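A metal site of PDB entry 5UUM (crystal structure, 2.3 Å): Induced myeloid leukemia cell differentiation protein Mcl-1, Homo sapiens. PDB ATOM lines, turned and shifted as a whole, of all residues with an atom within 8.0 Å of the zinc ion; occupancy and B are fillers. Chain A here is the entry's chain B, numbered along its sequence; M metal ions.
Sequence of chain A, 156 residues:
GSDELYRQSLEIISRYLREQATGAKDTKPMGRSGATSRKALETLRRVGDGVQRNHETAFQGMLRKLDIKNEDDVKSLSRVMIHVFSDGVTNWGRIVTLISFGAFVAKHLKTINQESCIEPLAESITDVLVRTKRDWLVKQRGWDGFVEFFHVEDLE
Three residues have an atom within 4 Å of the zinc ion: Glu 148, His 151 and Glu 153. The nearest printed residue that does not touch the zinc ion is Val 152 (5.9 Å).
The side-chain carboxylate (OE2) of Glu 153 binds the zinc ion, 1.9 Å away. The zinc ion is bound by ND1 of His 151 (2.2 Å). OE1 of Glu 148 binds the zinc ion. The zinc ion has three donor atoms within binding distance.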
ATOM      1  N   ASP A 144      15.090  18.530 -14.401  1.00  0.00           N
ATOM      2  CA  ASP A 144      13.928  18.396 -13.521  1.00  0.00           C
ATOM      3  C   ASP A 144      12.879  17.479 -14.148  1.00  0.00           C
ATOM      4  O   ASP A 144      12.301  16.632 -13.460  1.00  0.00           O
ATOM      5  CB  ASP A 144      13.341  19.774 -13.217  1.00  0.00           C
ATOM      6  CG  ASP A 144      14.277  20.649 -12.398  1.00  0.00           C
ATOM      7  OD1 ASP A 144      15.046  20.127 -11.568  1.00  0.00           O
ATOM      8  OD2 ASP A 144      14.241  21.890 -12.582  1.00  0.00           O
ATOM      9  N   VAL A 147      14.163  13.858 -13.973  1.00  0.00           N
ATOM     10  CA  VAL A 147      14.007  13.290 -12.635  1.00  0.00           C
ATOM     11  C   VAL A 147      12.566  12.860 -12.401  1.00  0.00           C
ATOM     12  O   VAL A 147      12.302  11.759 -11.920  1.00  0.00           O
ATOM     13  CB  VAL A 147      14.471  14.300 -11.569  1.00  0.00           C
ATOM     14  CG1 VAL A 147      14.121  13.812 -10.165  1.00  0.00           C
ATOM     15  CG2 VAL A 147      15.978  14.552 -11.676  1.00  0.00           C
ATOM     16  N   GLU A 148      11.614  13.734 -12.737  1.00  0.00           N
ATOM     17  CA  GLU A 148      10.212  13.438 -12.463  1.00  0.00           C
ATOM     18  C   GLU A 148       9.697  12.287 -13.319  1.00  0.00           C
ATOM     19  O   GLU A 148       8.854  11.505 -12.871  1.00  0.00           O
ATOM     20  CB  GLU A 148       9.361  14.690 -12.688  1.00  0.00           C
ATOM     21  CG  GLU A 148       9.605  15.786 -11.677  1.00  0.00           C
ATOM     22  CD  GLU A 148       9.456  15.301 -10.247  1.00  0.00           C
ATOM     23  OE1 GLU A 148       8.568  14.454  -9.997  1.00  0.00           O
ATOM     24  OE2 GLU A 148      10.230  15.746  -9.372  1.00  0.00           O
ATOM     25  N   PHE A 149      10.187  12.179 -14.560  1.00  0.00           N
ATOM     26  CA  PHE A 149       9.684  11.155 -15.451  1.00  0.00           C
ATOM     27  C   PHE A 149       9.952   9.758 -14.913  1.00  0.00           C
ATOM     28  O   PHE A 149       9.120   8.854 -15.061  1.00  0.00           O
ATOM     29  CB  PHE A 149      10.308  11.320 -16.838  1.00  0.00           C
ATOM     30  CG  PHE A 149       9.858  10.289 -17.832  1.00  0.00           C
ATOM     31  CD1 PHE A 149       8.647  10.417 -18.493  1.00  0.00           C
ATOM     32  CD2 PHE A 149      10.653   9.182 -18.109  1.00  0.00           C
ATOM     33  CE1 PHE A 149       8.236   9.463 -19.412  1.00  0.00           C
ATOM     34  CE2 PHE A 149      10.243   8.229 -19.014  1.00  0.00           C
ATOM     35  CZ  PHE A 149       9.035   8.381 -19.670  1.00  0.00           C
ATOM     36  N   PHE A 150      11.098   9.566 -14.255  1.00  0.00           N
ATOM     37  CA  PHE A 150      11.483   8.271 -13.716  1.00  0.00           C
ATOM     38  C   PHE A 150      11.256   8.152 -12.217  1.00  0.00           C
ATOM     39  O   PHE A 150      11.641   7.127 -11.633  1.00  0.00           O
ATOM     40  CB  PHE A 150      12.956   7.986 -14.031  1.00  0.00           C
ATOM     41  CG  PHE A 150      13.231   7.774 -15.494  1.00  0.00           C
ATOM     42  CD1 PHE A 150      12.780   6.629 -16.142  1.00  0.00           C
ATOM     43  CD2 PHE A 150      13.958   8.700 -16.224  1.00  0.00           C
ATOM     44  CE1 PHE A 150      13.034   6.427 -17.483  1.00  0.00           C
ATOM     45  CE2 PHE A 150      14.222   8.502 -17.567  1.00  0.00           C
ATOM     46  CZ  PHE A 150      13.761   7.362 -18.192  1.00  0.00           C
ATOM     47  N   HIS A 151      10.668   9.156 -11.576  1.00  0.00           N
ATOM     48  CA  HIS A 151      10.400   9.116 -10.145  1.00  0.00           C
ATOM     49  C   HIS A 151       9.070   8.417  -9.901  1.00  0.00           C
ATOM     50  O   HIS A 151       8.007   8.972 -10.189  1.00  0.00           O
ATOM     51  CB  HIS A 151      10.378  10.528  -9.571  1.00  0.00           C
ATOM     52  CG  HIS A 151      10.175  10.571  -8.082  1.00  0.00           C
ATOM     53  ND1 HIS A 151       9.490  11.582  -7.456  1.00  0.00           N
ATOM     54  CD2 HIS A 151      10.574   9.720  -7.111  1.00  0.00           C
ATOM     55  CE1 HIS A 151       9.471  11.355  -6.155  1.00  0.00           C
ATOM     56  NE2 HIS A 151      10.118  10.235  -5.912  1.00  0.00           N
ATOM     57  N   VAL A 152       9.129   7.193  -9.378  1.00  0.00           N
ATOM     58  CA  VAL A 152       7.901   6.465  -9.047  1.00  0.00           C
ATOM     59  C   VAL A 152       7.351   7.019  -7.745  1.00  0.00           C
ATOM     60  O   VAL A 152       8.038   7.035  -6.719  1.00  0.00           O
ATOM     61  CB  VAL A 152       8.152   4.955  -8.968  1.00  0.00           C
ATOM     62  CG1 VAL A 152       9.105   4.600  -7.828  1.00  0.00           C
ATOM     63  CG2 VAL A 152       6.837   4.201  -8.826  1.00  0.00           C
ATOM     64  N   GLU A 153       6.101   7.484  -7.787  1.00  0.00           N
ATOM     65  CA  GLU A 153       5.542   8.215  -6.658  1.00  0.00           C
ATOM     66  C   GLU A 153       5.159   7.275  -5.514  1.00  0.00           C
ATOM     67  O   GLU A 153       5.273   7.656  -4.342  1.00  0.00           O
ATOM     68  CB  GLU A 153       4.331   9.031  -7.124  1.00  0.00           C
ATOM     69  CG  GLU A 153       4.674  10.125  -8.131  1.00  0.00           C
ATOM     70  CD  GLU A 153       5.697  11.101  -7.593  1.00  0.00           C
ATOM     71  OE1 GLU A 153       5.811  11.220  -6.352  1.00  0.00           O
ATOM     72  OE2 GLU A 153       6.387  11.765  -8.401  1.00  0.00           O
ATOM     73  N   ASP A 154       4.711   6.067  -5.827  1.00  0.00           N
ATOM     74  CA  ASP A 154       4.263   5.120  -4.811  1.00  0.00           C
ATOM     75  C   ASP A 154       4.922   3.767  -5.067  1.00  0.00           C
ATOM     76  O   ASP A 154       4.744   3.175  -6.134  1.00  0.00           O
ATOM     77  CB  ASP A 154       2.740   4.989  -4.815  1.00  0.00           C
ATOM     78  CG  ASP A 154       2.219   4.164  -3.663  1.00  0.00           C
ATOM     79  OD1 ASP A 154       3.044   3.648  -2.874  1.00  0.00           O
ATOM     80  OD2 ASP A 154       0.981   4.039  -3.534  1.00  0.00           O
HETATM   81 ZN    ZN M   1       7.912  12.913  -8.071  1.00  0.00          ZN
